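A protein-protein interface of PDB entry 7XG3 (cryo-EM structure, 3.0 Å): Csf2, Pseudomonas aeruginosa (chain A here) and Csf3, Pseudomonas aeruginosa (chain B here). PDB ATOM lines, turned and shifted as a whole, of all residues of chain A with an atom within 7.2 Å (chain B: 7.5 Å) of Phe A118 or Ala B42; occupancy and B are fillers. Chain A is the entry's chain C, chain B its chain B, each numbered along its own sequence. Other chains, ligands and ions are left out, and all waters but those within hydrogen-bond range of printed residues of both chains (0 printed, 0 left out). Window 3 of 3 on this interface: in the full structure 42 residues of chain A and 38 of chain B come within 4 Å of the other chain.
Ser A116 touches none of the printed residues of chain B.
Phe A118 touches four residues of chain B.
Glu A120 touches none of the printed residues of chain B.
Printed residues of chain B within 4 Å of Arg A125: Arg B36 (3.9 Å) and Asp B41 (3.2 Å).
Of chain A, only Phe A118 and Ala A122 come within 4 Å of Ala B42.
Printed residues of chain A within 4 Å of Pro B45: Phe A118.
The nearest residue of chain B that does not touch Phe A118 is Asp B41 (4.4 Å).
The nearest residue of chain A that does not touch Ala B42 is Asp A119 (4.4 Å).
The nearest printed residue of chain B that does not touch Arg A266 is Gly B40 (4.2 Å).
Among the printed residues, merely in contact across the chains: Phe A118 with Asn B44 (3.2 Å), Ala A122 with Asp B41 (3.3 Å), Phe A118 with Ile B43 (3.4 Å), Ala A122 with Ala B42 (3.7 Å), Phe A118 with Ala B42 (3.8 Å), Phe A118 with Pro B45 (3.9 Å) and Arg A125 with Arg B36 (3.9 Å).
Of the 11 printed residues of chain A, 4 touch a printed residue of chain B.
Hydrophobic or aromatic side chains of chain A within 4 Å of the printed part of chain B: Phe A118 and Ala A122.
Of the 11 printed residues of chain B, 6 touch a printed residue of chain A.
Printed residues of chain B that touch a printed residue of chain A: Arg B36, Asp B41, Ala B42, Ile B43, Asn B44 and Pro B45.
Hydrophobic or aromatic side chains of chain B within 4 Å of the printed part of chain A: Ala B42 and Pro B45.
Along chain B the printed residues that touch a printed residue of chain A span positions 36 to 45.
Among the printed residues, 10 pairs touch across the chains.
Among the printed residues, Asp or Glu carboxylates within 4 Å of a Lys or Arg side-chain nitrogen of the other chain: Arg A125 with Asp B41 (3.9 Å) and Arg A266 with Asp B41 (3.8 Å).
O of Arg B36 sits close to NH1 of Arg A266 (3.4 Å).
OD1 of Asp B41 lies within salt-bridge range of NE of Arg A125, 3.9 Å away.
The side-chain carboxylate of Asp B41 lies within salt-bridge range of the guanidinium group of Arg A266 (3.8 Å).
NH1 of Arg B36 lies within salt-bridge range of OD1 of Asp B41 (2.5 Å).
The side-chain amide oxygen (OD1) of Asn B44 lies close to the backbone NH (N) of Arg B46 (3.2 Å).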
ATOM      1  N   SER A 116     -23.324  11.208  16.272  1.00  0.00           N
ATOM      2  CA  SER A 116     -22.799  10.028  15.600  1.00  0.00           C
ATOM      3  C   SER A 116     -22.200   9.097  16.639  1.00  0.00           C
ATOM      4  O   SER A 116     -21.205   9.441  17.284  1.00  0.00           O
ATOM      5  CB  SER A 116     -21.752  10.413  14.552  1.00  0.00           C
ATOM      6  OG  SER A 116     -22.330  11.170  13.505  1.00  0.00           O
ATOM      7  N   SER A 117     -22.812   7.928  16.808  1.00  0.00           N
ATOM      8  CA  SER A 117     -22.221   6.899  17.649  1.00  0.00           C
ATOM      9  C   SER A 117     -21.002   6.306  16.957  1.00  0.00           C
ATOM     10  O   SER A 117     -20.852   6.390  15.737  1.00  0.00           O
ATOM     11  CB  SER A 117     -23.238   5.803  17.958  1.00  0.00           C
ATOM     12  OG  SER A 117     -23.372   4.908  16.869  1.00  0.00           O
ATOM     13  N   PHE A 118     -20.119   5.706  17.755  1.00  0.00           N
ATOM     14  CA  PHE A 118     -18.862   5.198  17.215  1.00  0.00           C
ATOM     15  C   PHE A 118     -19.088   3.964  16.350  1.00  0.00           C
ATOM     16  O   PHE A 118     -18.366   3.742  15.369  1.00  0.00           O
ATOM     17  CB  PHE A 118     -17.900   4.906  18.361  1.00  0.00           C
ATOM     18  CG  PHE A 118     -17.954   5.932  19.453  1.00  0.00           C
ATOM     19  CD1 PHE A 118     -17.443   7.203  19.250  1.00  0.00           C
ATOM     20  CD2 PHE A 118     -18.536   5.632  20.675  1.00  0.00           C
ATOM     21  CE1 PHE A 118     -17.500   8.156  20.250  1.00  0.00           C
ATOM     22  CE2 PHE A 118     -18.596   6.580  21.680  1.00  0.00           C
ATOM     23  CZ  PHE A 118     -18.080   7.843  21.465  1.00  0.00           C
ATOM     24  N   ASP A 119     -20.103   3.163  16.685  1.00  0.00           N
ATOM     25  CA  ASP A 119     -20.457   2.019  15.850  1.00  0.00           C
ATOM     26  C   ASP A 119     -21.015   2.462  14.503  1.00  0.00           C
ATOM     27  O   ASP A 119     -20.674   1.882  13.465  1.00  0.00           O
ATOM     28  CB  ASP A 119     -21.459   1.127  16.581  1.00  0.00           C
ATOM     29  CG  ASP A 119     -21.419  -0.313  16.103  1.00  0.00           C
ATOM     30  OD1 ASP A 119     -20.710  -0.600  15.114  1.00  0.00           O
ATOM     31  OD2 ASP A 119     -22.097  -1.162  16.718  1.00  0.00           O
ATOM     32  N   GLU A 120     -21.858   3.498  14.489  1.00  0.00           N
ATOM     33  CA  GLU A 120     -22.377   3.972  13.210  1.00  0.00           C
ATOM     34  C   GLU A 120     -21.319   4.753  12.436  1.00  0.00           C
ATOM     35  O   GLU A 120     -21.331   4.735  11.200  1.00  0.00           O
ATOM     36  CB  GLU A 120     -23.664   4.784  13.418  1.00  0.00           C
ATOM     37  CG  GLU A 120     -23.510   6.232  13.853  1.00  0.00           C
ATOM     38  CD  GLU A 120     -24.821   6.830  14.333  1.00  0.00           C
ATOM     39  OE1 GLU A 120     -25.831   6.718  13.609  1.00  0.00           O
ATOM     40  OE2 GLU A 120     -24.846   7.401  15.444  1.00  0.00           O
ATOM     41  N   ILE A 121     -20.368   5.381  13.140  1.00  0.00           N
ATOM     42  CA  ILE A 121     -19.206   5.989  12.489  1.00  0.00           C
ATOM     43  C   ILE A 121     -18.393   4.919  11.769  1.00  0.00           C
ATOM     44  O   ILE A 121     -17.989   5.088  10.611  1.00  0.00           O
ATOM     45  CB  ILE A 121     -18.358   6.756  13.524  1.00  0.00           C
ATOM     46  CG1 ILE A 121     -18.932   8.153  13.757  1.00  0.00           C
ATOM     47  CG2 ILE A 121     -16.897   6.874  13.100  1.00  0.00           C
ATOM     48  CD1 ILE A 121     -18.244   8.916  14.866  1.00  0.00           C
ATOM     49  N   ALA A 122     -18.189   3.779  12.438  1.00  0.00           N
ATOM     50  CA  ALA A 122     -17.469   2.665  11.829  1.00  0.00           C
ATOM     51  C   ALA A 122     -18.239   2.062  10.660  1.00  0.00           C
ATOM     52  O   ALA A 122     -17.638   1.688   9.646  1.00  0.00           O
ATOM     53  CB  ALA A 122     -17.180   1.597  12.879  1.00  0.00           C
ATOM     54  N   THR A 123     -19.565   1.956  10.774  1.00  0.00           N
ATOM     55  CA  THR A 123     -20.320   1.304   9.708  1.00  0.00           C
ATOM     56  C   THR A 123     -20.550   2.234   8.521  1.00  0.00           C
ATOM     57  O   THR A 123     -20.915   1.764   7.437  1.00  0.00           O
ATOM     58  CB  THR A 123     -21.650   0.753  10.240  1.00  0.00           C
ATOM     59  OG1 THR A 123     -22.070  -0.342   9.417  1.00  0.00           O
ATOM     60  CG2 THR A 123     -22.745   1.809  10.231  1.00  0.00           C
ATOM     61  N   MET A 124     -20.336   3.545   8.689  1.00  0.00           N
ATOM     62  CA  MET A 124     -20.418   4.417   7.521  1.00  0.00           C
ATOM     63  C   MET A 124     -19.047   4.711   6.929  1.00  0.00           C
ATOM     64  O   MET A 124     -18.946   5.024   5.737  1.00  0.00           O
ATOM     65  CB  MET A 124     -21.147   5.716   7.862  1.00  0.00           C
ATOM     66  CG  MET A 124     -22.585   5.546   8.348  1.00  0.00           C
ATOM     67  SD  MET A 124     -23.865   5.516   7.071  1.00  0.00           S
ATOM     68  CE  MET A 124     -23.864   3.822   6.480  1.00  0.00           C
ATOM     69  N   ARG A 125     -17.981   4.613   7.726  1.00  0.00           N
ATOM     70  CA  ARG A 125     -16.653   4.762   7.145  1.00  0.00           C
ATOM     71  C   ARG A 125     -16.215   3.536   6.356  1.00  0.00           C
ATOM     72  O   ARG A 125     -15.282   3.641   5.555  1.00  0.00           O
ATOM     73  CB  ARG A 125     -15.617   5.068   8.224  1.00  0.00           C
ATOM     74  CG  ARG A 125     -15.641   6.488   8.741  1.00  0.00           C
ATOM     75  CD  ARG A 125     -14.720   6.661   9.936  1.00  0.00           C
ATOM     76  NE  ARG A 125     -13.369   7.044   9.544  1.00  0.00           N
ATOM     77  CZ  ARG A 125     -12.716   8.087  10.036  1.00  0.00           C
ATOM     78  NH1 ARG A 125     -13.257   8.867  10.958  1.00  0.00           N
ATOM     79  NH2 ARG A 125     -11.489   8.352   9.596  1.00  0.00           N
ATOM     80  N   ARG A 266      -6.399   4.103   6.038  1.00  0.00           N
ATOM     81  CA  ARG A 266      -6.889   2.761   6.342  1.00  0.00           C
ATOM     82  C   ARG A 266      -8.104   2.348   5.503  1.00  0.00           C
ATOM     83  O   ARG A 266      -9.221   2.258   6.022  1.00  0.00           O
ATOM     84  CB  ARG A 266      -7.192   2.611   7.827  1.00  0.00           C
ATOM     85  CG  ARG A 266      -6.247   3.346   8.769  1.00  0.00           C
ATOM     86  CD  ARG A 266      -6.891   3.519  10.130  1.00  0.00           C
ATOM     87  NE  ARG A 266      -8.000   4.466  10.077  1.00  0.00           N
ATOM     88  CZ  ARG A 266      -9.208   4.237  10.575  1.00  0.00           C
ATOM     89  NH1 ARG A 266      -9.511   3.086  11.151  1.00  0.00           N
ATOM     90  NH2 ARG A 266     -10.137   5.183  10.482  1.00  0.00           N
ATOM     91  N   ARG B  36      -6.872   3.785  15.911  1.00  0.00           N
ATOM     92  CA  ARG B  36      -7.756   3.320  14.849  1.00  0.00           C
ATOM     93  C   ARG B  36      -7.094   2.226  14.027  1.00  0.00           C
ATOM     94  O   ARG B  36      -7.766   1.310  13.536  1.00  0.00           O
ATOM     95  CB  ARG B  36      -8.172   4.488  13.957  1.00  0.00           C
ATOM     96  CG  ARG B  36      -9.200   5.412  14.581  1.00  0.00           C
ATOM     97  CD  ARG B  36      -9.641   6.494  13.614  1.00  0.00           C
ATOM     98  NE  ARG B  36     -10.659   7.355  14.199  1.00  0.00           N
ATOM     99  CZ  ARG B  36     -11.957   7.085  14.211  1.00  0.00           C
ATOM    100  NH1 ARG B  36     -12.437   5.979  13.668  1.00  0.00           N
ATOM    101  NH2 ARG B  36     -12.792   7.944  14.786  1.00  0.00           N
ATOM    102  N   HIS B  39      -6.735  -0.973  16.929  1.00  0.00           N
ATOM    103  CA  HIS B  39      -7.975  -1.647  17.317  1.00  0.00           C
ATOM    104  C   HIS B  39      -8.906  -1.869  16.133  1.00  0.00           C
ATOM    105  O   HIS B  39      -9.306  -3.003  15.853  1.00  0.00           O
ATOM    106  CB  HIS B  39      -8.740  -0.864  18.399  1.00  0.00           C
ATOM    107  CG  HIS B  39      -7.948  -0.535  19.627  1.00  0.00           C
ATOM    108  ND1 HIS B  39      -6.706  -1.066  19.896  1.00  0.00           N
ATOM    109  CD2 HIS B  39      -8.238   0.280  20.669  1.00  0.00           C
ATOM    110  CE1 HIS B  39      -6.265  -0.594  21.047  1.00  0.00           C
ATOM    111  NE2 HIS B  39      -7.175   0.226  21.537  1.00  0.00           N
ATOM    112  N   GLY B  40      -9.259  -0.799  15.439  1.00  0.00           N
ATOM    113  CA  GLY B  40     -10.274  -0.801  14.417  1.00  0.00           C
ATOM    114  C   GLY B  40     -10.985   0.527  14.391  1.00  0.00           C
ATOM    115  O   GLY B  40     -10.505   1.532  14.923  1.00  0.00           O
ATOM    116  N   ASP B  41     -12.170   0.540  13.785  1.00  0.00           N
ATOM    117  CA  ASP B  41     -12.828   1.813  13.520  1.00  0.00           C
ATOM    118  C   ASP B  41     -13.811   2.184  14.627  1.00  0.00           C
ATOM    119  O   ASP B  41     -14.040   3.372  14.886  1.00  0.00           O
ATOM    120  CB  ASP B  41     -13.525   1.750  12.168  1.00  0.00           C
ATOM    121  CG  ASP B  41     -13.786   3.115  11.586  1.00  0.00           C
ATOM    122  OD1 ASP B  41     -13.330   4.121  12.171  1.00  0.00           O
ATOM    123  OD2 ASP B  41     -14.434   3.175  10.529  1.00  0.00           O
ATOM    124  N   ALA B  42     -14.402   1.190  15.290  1.00  0.00           N
ATOM    125  CA  ALA B  42     -15.436   1.437  16.296  1.00  0.00           C
ATOM    126  C   ALA B  42     -14.787   1.606  17.667  1.00  0.00           C
ATOM    127  O   ALA B  42     -14.773   0.700  18.503  1.00  0.00           O
ATOM    128  CB  ALA B  42     -16.457   0.307  16.305  1.00  0.00           C
ATOM    129  N   ILE B  43     -14.241   2.801  17.901  1.00  0.00           N
ATOM    130  CA  ILE B  43     -13.657   3.161  19.186  1.00  0.00           C
ATOM    131  C   ILE B  43     -14.076   4.581  19.541  1.00  0.00           C
ATOM    132  O   ILE B  43     -14.586   5.332  18.710  1.00  0.00           O
ATOM    133  CB  ILE B  43     -12.120   3.055  19.198  1.00  0.00           C
ATOM    134  CG1 ILE B  43     -11.537   3.716  17.949  1.00  0.00           C
ATOM    135  CG2 ILE B  43     -11.677   1.598  19.353  1.00  0.00           C
ATOM    136  CD1 ILE B  43     -10.082   3.419  17.724  1.00  0.00           C
ATOM    137  N   ASN B  44     -13.839   4.940  20.800  1.00  0.00           N
ATOM    138  CA  ASN B  44     -14.079   6.291  21.279  1.00  0.00           C
ATOM    139  C   ASN B  44     -12.789   7.085  21.164  1.00  0.00           C
ATOM    140  O   ASN B  44     -11.787   6.708  21.785  1.00  0.00           O
ATOM    141  CB  ASN B  44     -14.566   6.270  22.726  1.00  0.00           C
ATOM    142  CG  ASN B  44     -15.011   7.637  23.223  1.00  0.00           C
ATOM    143  OD1 ASN B  44     -15.147   8.586  22.451  1.00  0.00           O
ATOM    144  ND2 ASN B  44     -15.241   7.739  24.526  1.00  0.00           N
ATOM    145  N   PRO B  45     -12.758   8.174  20.390  1.00  0.00           N
ATOM    146  CA  PRO B  45     -11.552   9.020  20.358  1.00  0.00           C
ATOM    147  C   PRO B  45     -11.269   9.738  21.670  1.00  0.00           C
ATOM    148  O   PRO B  45     -10.141  10.204  21.877  1.00  0.00           O
ATOM    149  CB  PRO B  45     -11.853  10.010  19.224  1.00  0.00           C
ATOM    150  CG  PRO B  45     -12.891   9.337  18.389  1.00  0.00           C
ATOM    151  CD  PRO B  45     -13.728   8.555  19.349  1.00  0.00           C
ATOM    152  N   ARG B  46     -12.259   9.844  22.562  1.00  0.00           N
ATOM    153  CA  ARG B  46     -12.031  10.391  23.894  1.00  0.00           C
ATOM    154  C   ARG B  46     -11.130   9.503  24.745  1.00  0.00           C
ATOM    155  O   ARG B  46     -10.473  10.005  25.665  1.00  0.00           O
ATOM    156  CB  ARG B  46     -13.377  10.618  24.594  1.00  0.00           C
ATOM    157  CG  ARG B  46     -13.337  11.487  25.856  1.00  0.00           C
ATOM    158  CD  ARG B  46     -13.070  12.957  25.562  1.00  0.00           C
ATOM    159  NE  ARG B  46     -13.782  13.436  24.385  1.00  0.00           N
ATOM    160  CZ  ARG B  46     -14.022  14.715  24.125  1.00  0.00           C
ATOM    161  NH1 ARG B  46     -13.636  15.673  24.952  1.00  0.00           N
ATOM    162  NH2 ARG B  46     -14.664  15.039  23.008  1.00  0.00           N
ATOM    163  N   ASP B  47     -11.058   8.204  24.442  1.00  0.00           N
ATOM    164  CA  ASP B  47     -10.303   7.284  25.286  1.00  0.00           C
ATOM    165  C   ASP B  47      -8.798   7.458  25.115  1.00  0.00           C
ATOM    166  O   ASP B  47      -8.053   7.451  26.102  1.00  0.00           O
ATOM    167  CB  ASP B  47     -10.702   5.843  24.973  1.00  0.00           C
ATOM    168  CG  ASP B  47     -12.032   5.460  25.584  1.00  0.00           C
ATOM    169  OD1 ASP B  47     -12.538   6.223  26.434  1.00  0.00           O
ATOM    170  OD2 ASP B  47     -12.568   4.394  25.218  1.00  0.00           O
ATOM    171  N   TYR B  48      -8.332   7.628  23.878  1.00  0.00           N
ATOM    172  CA  TYR B  48      -6.915   7.489  23.579  1.00  0.00           C
ATOM    173  C   TYR B  48      -6.214   8.789  23.218  1.00  0.00           C
ATOM    174  O   TYR B  48      -4.988   8.786  23.102  1.00  0.00           O
ATOM    175  CB  TYR B  48      -6.677   6.480  22.437  1.00  0.00           C
ATOM    176  CG  TYR B  48      -7.617   5.289  22.387  1.00  0.00           C
ATOM    177  CD1 TYR B  48      -8.859   5.364  21.758  1.00  0.00           C
ATOM    178  CD2 TYR B  48      -7.268   4.093  23.001  1.00  0.00           C
ATOM    179  CE1 TYR B  48      -9.712   4.275  21.729  1.00  0.00           C
ATOM    180  CE2 TYR B  48      -8.119   3.003  22.978  1.00  0.00           C
ATOM    181  CZ  TYR B  48      -9.336   3.100  22.339  1.00  0.00           C
ATOM    182  OH  TYR B  48     -10.186   2.021  22.317  1.00  0.00           O
